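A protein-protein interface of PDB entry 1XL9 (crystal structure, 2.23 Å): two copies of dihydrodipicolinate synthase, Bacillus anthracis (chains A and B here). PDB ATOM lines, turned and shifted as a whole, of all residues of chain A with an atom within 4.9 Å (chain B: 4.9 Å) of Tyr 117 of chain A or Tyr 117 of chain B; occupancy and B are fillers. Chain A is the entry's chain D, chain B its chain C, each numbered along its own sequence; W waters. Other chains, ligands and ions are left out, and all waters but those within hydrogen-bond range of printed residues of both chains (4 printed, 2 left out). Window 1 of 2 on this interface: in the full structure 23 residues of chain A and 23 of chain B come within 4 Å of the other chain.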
ATOM      1  N   SER A  90     -22.738  -3.878 -14.164  1.00  0.00           N
ATOM      2  CA  SER A  90     -22.980  -4.681 -15.330  1.00  0.00           C
ATOM      3  C   SER A  90     -21.636  -5.191 -15.885  1.00  0.00           C
ATOM      4  O   SER A  90     -20.557  -5.013 -15.279  1.00  0.00           O
ATOM      5  CB  SER A  90     -23.810  -3.887 -16.395  1.00  0.00           C
ATOM      6  OG  SER A  90     -23.128  -2.739 -16.879  1.00  0.00           O
ATOM      7  N   ASN A  91     -21.724  -5.855 -17.034  1.00  0.00           N
ATOM      8  CA  ASN A  91     -20.532  -6.161 -17.823  1.00  0.00           C
ATOM      9  C   ASN A  91     -19.876  -4.957 -18.549  1.00  0.00           C
ATOM     10  O   ASN A  91     -18.811  -5.118 -19.166  1.00  0.00           O
ATOM     11  CB  ASN A  91     -20.810  -7.330 -18.794  1.00  0.00           C
ATOM     12  CG  ASN A  91     -21.757  -6.982 -19.897  1.00  0.00           C
ATOM     13  OD1 ASN A  91     -21.912  -7.758 -20.841  1.00  0.00           O
ATOM     14  ND2 ASN A  91     -22.401  -5.824 -19.804  1.00  0.00           N
ATOM     15  N   VAL A 114     -21.454  -6.957  -9.838  1.00  0.00           N
ATOM     16  CA  VAL A 114     -21.264  -8.303 -10.311  1.00  0.00           C
ATOM     17  C   VAL A 114     -20.056  -8.399 -11.240  1.00  0.00           C
ATOM     18  O   VAL A 114     -19.801  -7.500 -12.039  1.00  0.00           O
ATOM     19  CB  VAL A 114     -22.544  -8.815 -11.038  1.00  0.00           C
ATOM     20  CG1 VAL A 114     -22.743  -8.084 -12.400  1.00  0.00           C
ATOM     21  CG2 VAL A 114     -22.478 -10.329 -11.212  1.00  0.00           C
ATOM     22  N   ALA A 115     -19.290  -9.484 -11.082  1.00  0.00           N
ATOM     23  CA  ALA A 115     -18.329  -9.961 -12.086  1.00  0.00           C
ATOM     24  C   ALA A 115     -18.970  -9.911 -13.489  1.00  0.00           C
ATOM     25  O   ALA A 115     -20.005 -10.606 -13.709  1.00  0.00           O
ATOM     26  CB  ALA A 115     -17.947 -11.412 -11.770  1.00  0.00           C
ATOM     27  N   PRO A 116     -18.358  -9.133 -14.428  1.00  0.00           N
ATOM     28  CA  PRO A 116     -18.857  -9.001 -15.782  1.00  0.00           C
ATOM     29  C   PRO A 116     -19.132 -10.350 -16.439  1.00  0.00           C
ATOM     30  O   PRO A 116     -18.249 -11.224 -16.474  1.00  0.00           O
ATOM     31  CB  PRO A 116     -17.720  -8.300 -16.508  1.00  0.00           C
ATOM     32  CG  PRO A 116     -17.074  -7.480 -15.465  1.00  0.00           C
ATOM     33  CD  PRO A 116     -17.127  -8.323 -14.247  1.00  0.00           C
ATOM     34  N   TYR A 117     -20.349 -10.467 -16.966  1.00  0.00           N
ATOM     35  CA  TYR A 117     -20.841 -11.666 -17.641  1.00  0.00           C
ATOM     36  C   TYR A 117     -20.574 -11.441 -19.122  1.00  0.00           C
ATOM     37  O   TYR A 117     -20.218 -10.282 -19.545  1.00  0.00           O
ATOM     38  CB  TYR A 117     -22.338 -11.871 -17.365  1.00  0.00           C
ATOM     39  CG  TYR A 117     -23.129 -10.589 -17.329  1.00  0.00           C
ATOM     40  CD1 TYR A 117     -23.446  -9.984 -16.129  1.00  0.00           C
ATOM     41  CD2 TYR A 117     -23.461  -9.915 -18.500  1.00  0.00           C
ATOM     42  CE1 TYR A 117     -24.088  -8.733 -16.094  1.00  0.00           C
ATOM     43  CE2 TYR A 117     -24.120  -8.665 -18.478  1.00  0.00           C
ATOM     44  CZ  TYR A 117     -24.431  -8.097 -17.266  1.00  0.00           C
ATOM     45  OH  TYR A 117     -25.114  -6.907 -17.221  1.00  0.00           O
ATOM     46  N   TYR A 118     -20.685 -12.542 -19.894  1.00  0.00           N
ATOM     47  CA  TYR A 118     -20.672 -12.550 -21.378  1.00  0.00           C
ATOM     48  C   TYR A 118     -19.353 -12.154 -22.064  1.00  0.00           C
ATOM     49  O   TYR A 118     -18.917 -12.894 -22.954  1.00  0.00           O
ATOM     50  CB  TYR A 118     -21.813 -11.713 -21.943  1.00  0.00           C
ATOM     51  CG  TYR A 118     -22.037 -11.881 -23.422  1.00  0.00           C
ATOM     52  CD1 TYR A 118     -22.332 -13.144 -23.990  1.00  0.00           C
ATOM     53  CD2 TYR A 118     -21.993 -10.777 -24.271  1.00  0.00           C
ATOM     54  CE1 TYR A 118     -22.541 -13.281 -25.382  1.00  0.00           C
ATOM     55  CE2 TYR A 118     -22.222 -10.908 -25.652  1.00  0.00           C
ATOM     56  CZ  TYR A 118     -22.487 -12.147 -26.201  1.00  0.00           C
ATOM     57  OH  TYR A 118     -22.697 -12.199 -27.573  1.00  0.00           O
ATOM     58  N   ASN A 119     -18.714 -11.026 -21.649  1.00  0.00           N
ATOM     59  CA  ASN A 119     -17.431 -10.633 -22.255  1.00  0.00           C
ATOM     60  C   ASN A 119     -16.194 -11.278 -21.695  1.00  0.00           C
ATOM     61  O   ASN A 119     -15.129 -11.117 -22.302  1.00  0.00           O
ATOM     62  CB  ASN A 119     -17.232  -9.102 -22.387  1.00  0.00           C
ATOM     63  CG  ASN A 119     -17.453  -8.320 -21.098  1.00  0.00           C
ATOM     64  OD1 ASN A 119     -17.650  -8.883 -20.044  1.00  0.00           O
ATOM     65  ND2 ASN A 119     -17.392  -6.969 -21.202  1.00  0.00           N
ATOM     66  N   LYS A 120     -16.318 -12.017 -20.576  1.00  0.00           N
ATOM     67  CA  LYS A 120     -15.219 -12.834 -20.020  1.00  0.00           C
ATOM     68  C   LYS A 120     -13.877 -12.096 -19.777  1.00  0.00           C
ATOM     69  O   LYS A 120     -12.838 -12.449 -20.358  1.00  0.00           O
ATOM     70  CB  LYS A 120     -14.983 -14.113 -20.868  1.00  0.00           C
ATOM     71  CG  LYS A 120     -16.236 -15.017 -20.993  1.00  0.00           C
ATOM     72  CD  LYS A 120     -15.950 -16.534 -20.789  1.00  0.00           C
ATOM     73  CE  LYS A 120     -14.990 -17.169 -21.827  1.00  0.00           C
ATOM     74  NZ  LYS A 120     -15.258 -16.949 -23.293  1.00  0.00           N
ATOM     75  N   ARG A 149     -23.371 -17.814 -13.294  1.00  0.00           N
ATOM     76  CA  ARG A 149     -23.991 -16.905 -14.259  1.00  0.00           C
ATOM     77  C   ARG A 149     -22.981 -16.166 -15.151  1.00  0.00           C
ATOM     78  O   ARG A 149     -23.276 -15.937 -16.329  1.00  0.00           O
ATOM     79  CB  ARG A 149     -24.922 -15.913 -13.540  1.00  0.00           C
ATOM     80  CG  ARG A 149     -25.994 -16.627 -12.688  1.00  0.00           C
ATOM     81  CD  ARG A 149     -27.010 -15.713 -11.963  1.00  0.00           C
ATOM     82  NE  ARG A 149     -28.238 -15.705 -12.738  1.00  0.00           N
ATOM     83  CZ  ARG A 149     -29.385 -16.284 -12.414  1.00  0.00           C
ATOM     84  NH1 ARG A 149     -29.598 -16.859 -11.246  1.00  0.00           N
ATOM     85  NH2 ARG A 149     -30.364 -16.216 -13.281  1.00  0.00           N
ATOM     86  N   SER A 150     -21.804 -15.795 -14.601  1.00  0.00           N
ATOM     87  CA  SER A 150     -20.785 -15.040 -15.362  1.00  0.00           C
ATOM     88  C   SER A 150     -19.677 -15.902 -15.992  1.00  0.00           C
ATOM     89  O   SER A 150     -18.938 -15.428 -16.817  1.00  0.00           O
ATOM     90  CB  SER A 150     -20.141 -13.952 -14.481  1.00  0.00           C
ATOM     91  OG  SER A 150     -21.105 -13.005 -14.025  1.00  0.00           O
ATOM     92  N   SER B  90     -29.719  -9.526 -27.511  1.00  0.00           N
ATOM     93  CA  SER B  90     -29.212  -9.446 -26.135  1.00  0.00           C
ATOM     94  C   SER B  90     -30.009 -10.423 -25.253  1.00  0.00           C
ATOM     95  O   SER B  90     -30.765 -11.259 -25.781  1.00  0.00           O
ATOM     96  CB  SER B  90     -29.312  -7.999 -25.619  1.00  0.00           C
ATOM     97  OG  SER B  90     -30.659  -7.557 -25.465  1.00  0.00           O
ATOM     98  N   ASN B  91     -29.841 -10.306 -23.933  1.00  0.00           N
ATOM     99  CA  ASN B  91     -30.652 -11.069 -22.940  1.00  0.00           C
ATOM    100  C   ASN B  91     -32.046 -10.489 -22.524  1.00  0.00           C
ATOM    101  O   ASN B  91     -32.692 -10.992 -21.611  1.00  0.00           O
ATOM    102  CB  ASN B  91     -29.813 -11.440 -21.693  1.00  0.00           C
ATOM    103  CG  ASN B  91     -29.364 -10.227 -20.894  1.00  0.00           C
ATOM    104  OD1 ASN B  91     -28.796 -10.368 -19.787  1.00  0.00           O
ATOM    105  ND2 ASN B  91     -29.643  -9.030 -21.416  1.00  0.00           N
ATOM    106  N   VAL B 114     -27.934 -13.793 -30.354  1.00  0.00           N
ATOM    107  CA  VAL B 114     -27.321 -14.628 -29.312  1.00  0.00           C
ATOM    108  C   VAL B 114     -28.359 -15.273 -28.357  1.00  0.00           C
ATOM    109  O   VAL B 114     -29.431 -14.713 -28.101  1.00  0.00           O
ATOM    110  CB  VAL B 114     -26.283 -13.883 -28.498  1.00  0.00           C
ATOM    111  CG1 VAL B 114     -26.934 -12.964 -27.481  1.00  0.00           C
ATOM    112  CG2 VAL B 114     -25.360 -14.868 -27.804  1.00  0.00           C
ATOM    113  N   ALA B 115     -28.004 -16.469 -27.878  1.00  0.00           N
ATOM    114  CA  ALA B 115     -28.643 -17.113 -26.744  1.00  0.00           C
ATOM    115  C   ALA B 115     -28.453 -16.237 -25.492  1.00  0.00           C
ATOM    116  O   ALA B 115     -27.313 -15.933 -25.113  1.00  0.00           O
ATOM    117  CB  ALA B 115     -28.029 -18.484 -26.508  1.00  0.00           C
ATOM    118  N   PRO B 116     -29.573 -15.838 -24.838  1.00  0.00           N
ATOM    119  CA  PRO B 116     -29.443 -14.870 -23.764  1.00  0.00           C
ATOM    120  C   PRO B 116     -28.463 -15.333 -22.699  1.00  0.00           C
ATOM    121  O   PRO B 116     -28.502 -16.516 -22.268  1.00  0.00           O
ATOM    122  CB  PRO B 116     -30.861 -14.782 -23.212  1.00  0.00           C
ATOM    123  CG  PRO B 116     -31.715 -15.166 -24.356  1.00  0.00           C
ATOM    124  CD  PRO B 116     -30.980 -16.250 -25.025  1.00  0.00           C
ATOM    125  N   TYR B 117     -27.596 -14.398 -22.305  1.00  0.00           N
ATOM    126  CA  TYR B 117     -26.544 -14.612 -21.328  1.00  0.00           C
ATOM    127  C   TYR B 117     -27.045 -14.110 -19.987  1.00  0.00           C
ATOM    128  O   TYR B 117     -27.987 -13.298 -19.907  1.00  0.00           O
ATOM    129  CB  TYR B 117     -25.263 -13.846 -21.732  1.00  0.00           C
ATOM    130  CG  TYR B 117     -25.567 -12.472 -22.278  1.00  0.00           C
ATOM    131  CD1 TYR B 117     -25.861 -12.291 -23.634  1.00  0.00           C
ATOM    132  CD2 TYR B 117     -25.613 -11.355 -21.444  1.00  0.00           C
ATOM    133  CE1 TYR B 117     -26.175 -11.038 -24.150  1.00  0.00           C
ATOM    134  CE2 TYR B 117     -25.935 -10.081 -21.960  1.00  0.00           C
ATOM    135  CZ  TYR B 117     -26.214  -9.946 -23.298  1.00  0.00           C
ATOM    136  OH  TYR B 117     -26.563  -8.731 -23.808  1.00  0.00           O
ATOM    137  N   TYR B 118     -26.417 -14.615 -18.937  1.00  0.00           N
ATOM    138  CA  TYR B 118     -26.534 -14.092 -17.567  1.00  0.00           C
ATOM    139  C   TYR B 118     -27.796 -14.484 -16.845  1.00  0.00           C
ATOM    140  O   TYR B 118     -27.714 -14.811 -15.670  1.00  0.00           O
ATOM    141  CB  TYR B 118     -26.306 -12.549 -17.498  1.00  0.00           C
ATOM    142  CG  TYR B 118     -26.277 -11.966 -16.093  1.00  0.00           C
ATOM    143  CD1 TYR B 118     -25.390 -12.445 -15.127  1.00  0.00           C
ATOM    144  CD2 TYR B 118     -27.121 -10.923 -15.742  1.00  0.00           C
ATOM    145  CE1 TYR B 118     -25.362 -11.910 -13.829  1.00  0.00           C
ATOM    146  CE2 TYR B 118     -27.116 -10.368 -14.454  1.00  0.00           C
ATOM    147  CZ  TYR B 118     -26.232 -10.858 -13.496  1.00  0.00           C
ATOM    148  OH  TYR B 118     -26.229 -10.299 -12.215  1.00  0.00           O
ATOM    149  N   ASN B 119     -28.942 -14.452 -17.521  1.00  0.00           N
ATOM    150  CA  ASN B 119     -30.242 -14.788 -16.896  1.00  0.00           C
ATOM    151  C   ASN B 119     -30.727 -16.260 -17.069  1.00  0.00           C
ATOM    152  O   ASN B 119     -31.828 -16.654 -16.589  1.00  0.00           O
ATOM    153  CB  ASN B 119     -31.358 -13.774 -17.282  1.00  0.00           C
ATOM    154  CG  ASN B 119     -31.599 -13.641 -18.802  1.00  0.00           C
ATOM    155  OD1 ASN B 119     -30.952 -14.299 -19.608  1.00  0.00           O
ATOM    156  ND2 ASN B 119     -32.546 -12.741 -19.188  1.00  0.00           N
ATOM    157  N   LYS B 120     -29.896 -17.056 -17.726  1.00  0.00           N
ATOM    158  CA  LYS B 120     -30.066 -18.490 -17.783  1.00  0.00           C
ATOM    159  C   LYS B 120     -31.541 -18.939 -18.086  1.00  0.00           C
ATOM    160  O   LYS B 120     -32.192 -19.563 -17.258  1.00  0.00           O
ATOM    161  CB  LYS B 120     -29.513 -19.129 -16.501  1.00  0.00           C
ATOM    162  CG  LYS B 120     -27.971 -19.112 -16.440  1.00  0.00           C
ATOM    163  CD  LYS B 120     -27.446 -20.089 -15.411  1.00  0.00           C
ATOM    164  CE  LYS B 120     -27.771 -19.618 -14.007  1.00  0.00           C
ATOM    165  NZ  LYS B 120     -28.098 -20.697 -13.000  1.00  0.00           N
ATOM    166  N   ARG B 149     -20.087 -18.494 -23.135  1.00  0.00           N
ATOM    167  CA  ARG B 149     -20.342 -17.109 -22.664  1.00  0.00           C
ATOM    168  C   ARG B 149     -21.723 -16.937 -22.040  1.00  0.00           C
ATOM    169  O   ARG B 149     -21.900 -16.150 -21.117  1.00  0.00           O
ATOM    170  CB  ARG B 149     -20.154 -16.086 -23.797  1.00  0.00           C
ATOM    171  CG  ARG B 149     -18.956 -16.370 -24.669  1.00  0.00           C
ATOM    172  CD  ARG B 149     -18.759 -15.361 -25.787  1.00  0.00           C
ATOM    173  NE  ARG B 149     -17.965 -14.299 -25.221  1.00  0.00           N
ATOM    174  CZ  ARG B 149     -16.687 -14.029 -25.493  1.00  0.00           C
ATOM    175  NH1 ARG B 149     -16.000 -14.644 -26.437  1.00  0.00           N
ATOM    176  NH2 ARG B 149     -16.106 -13.067 -24.806  1.00  0.00           N
ATOM    177  N   SER B 150     -22.698 -17.682 -22.538  1.00  0.00           N
ATOM    178  CA  SER B 150     -24.054 -17.614 -22.043  1.00  0.00           C
ATOM    179  C   SER B 150     -24.419 -18.735 -21.102  1.00  0.00           C
ATOM    180  O   SER B 150     -25.487 -18.689 -20.506  1.00  0.00           O
ATOM    181  CB  SER B 150     -25.017 -17.592 -23.231  1.00  0.00           C
ATOM    182  OG  SER B 150     -24.797 -16.437 -24.026  1.00  0.00           O
HETATM  183  O   HOH W   1     -32.623 -15.125 -14.140  1.00  0.00           O
HETATM  184  O   HOH W   2     -29.422 -20.072 -10.579  1.00  0.00           O
HETATM  185  O   HOH W   3     -23.932  -7.511 -22.868  1.00  0.00           O
HETATM  186  O   HOH W   4     -27.896  -8.121 -18.282  1.00  0.00           O
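Tyr 117 of chain A touches just these residues of chain B: Tyr 117 (3.9 Å) and Tyr 118 (3.3 Å). Of chain A, only Tyr 117 and Tyr 118 come within 4 Å of Tyr 117 of chain B. Of the printed residues of chain A, Lys 120 of chain B touches Arg 149. Printed residues of chain A within 4 Å of Tyr 118 of chain B: Val 114 (3.9 Å), Tyr 117 (3.3 Å) and Arg 149 (3.1 Å). Printed residues of chain B within 4 Å of Tyr 118 of chain A: Val 114, Tyr 117 and Arg 149. Pro 116 of chain A touches none of the printed residues of chain B. The nearest printed residue of chain B that does not touch Tyr 117 of chain A is Asn 91 of chain B (5.1 Å). The nearest printed residue of chain B that does not touch Asn 119 of chain A is Tyr 117 of chain B (6.9 Å).
The backbone carbonyl oxygen (O) of Tyr 118 of chain B sits at hydrogen-bond distance from the guanidinium group (NE) of Arg 149 of chain A (3.1 Å). The backbone carbonyl oxygen (O) of Tyr 118 of chain A sits at hydrogen-bond distance from the guanidinium group (NE) of Arg 149 of chain B, at 2.8 Å. The backbone carbonyl oxygen (O) of Asn 119 of chain A is in hydrogen-bond range of the guanidinium group (NH2) of Arg 149 of chain B (3.3 Å).
The backbone carbonyl oxygen (O) of Tyr 117 of chain B sits close to the side-chain amide oxygen (OD1) of Asn 91 of chain B, at 3.0 Å. ND2 of Asn 119 of chain B sits at hydrogen-bond distance from O of Asn 91 of chain B (3.0 Å). The side-chain amide oxygen (OD1) of Asn 119 of chain B lies close to the backbone carbonyl oxygen (O) of Tyr 117 of chain B (3.1 Å). The backbone carbonyl oxygen (O) of Tyr 117 of chain A sits close to the side-chain amide oxygen (OD1) of Asn 91 of chain A, at 3.3 Å. O of Asn 91 of chain A sits at hydrogen-bond distance from ND2 of Asn 119 of chain A, 3.1 Å away. O of Tyr 117 of chain A lies close to OD1 of Asn 119 of chain A, 3.0 Å away.
Tyr 117 of chain A touches Tyr 118 of chain B, and with the chains exchanged Tyr 118 of chain A touches Tyr 117 of chain B. Tyr 118 of chain A touches Arg 149 of chain B, and with the chains exchanged Arg 149 of chain A touches Tyr 118 of chain B. Asn 119 of chain A touches Arg 149 of chain B, and with the chains exchanged Arg 149 of chain A touches Asn 119 of chain B. Lys 120 of chain A touches Arg 149 of chain B, and with the chains exchanged Arg 149 of chain A touches Lys 120 of chain B. Positions printed for both chains: 90, 91, 114, 115, 116, 117, 118, 119, 120, 149 and 150. Of the 11 pairs that touch across the chains among the printed residues, 11 have their exchanged pair printed and touching as well.
Water W1 bridges NH2 of Arg 149 of chain A and O of Asn 119 of chain B. Water W2 lies within hydrogen-bond range of NZ of Lys 120 of chain B (2.8 Å) and NH1 of Arg 149 of chain A (3.3 Å). Water W4 bridges the side-chain amide oxygen (OD1) of Asn 91 of chain B (2.9 Å) and the side-chain hydroxyl (OH) of Tyr 117 of chain A (3.2 Å). Water W3 bridges OD1 of Asn 91 of chain A and OH of Tyr 117 of chain B.
Among the printed residues, merely in contact across the chains: Tyr 117 of chain A with Tyr 118 of chain B (3.3 Å), Arg 149 of chain A with Asn 119 of chain B (3.6 Å), Tyr 118 of chain A with Tyr 117 of chain B (3.6 Å), Arg 149 of chain A with Lys 120 of chain B (3.7 Å), Tyr 118 of chain A with Val 114 of chain B (3.8 Å), Val 114 of chain A with Tyr 118 of chain B (3.9 Å), Tyr 117 of chain A with Tyr 117 of chain B (3.9 Å) and Lys 120 of chain A with Arg 149 of chain B (3.9 Å).
Hydrophobic or aromatic side chains of chain B that line the printed part of chain A: Val 114, Tyr 117 and Tyr 118. Of the 11 printed residues of chain A, 6 touch a printed residue of chain B. Among the printed residues, 11 pairs touch across the chains.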
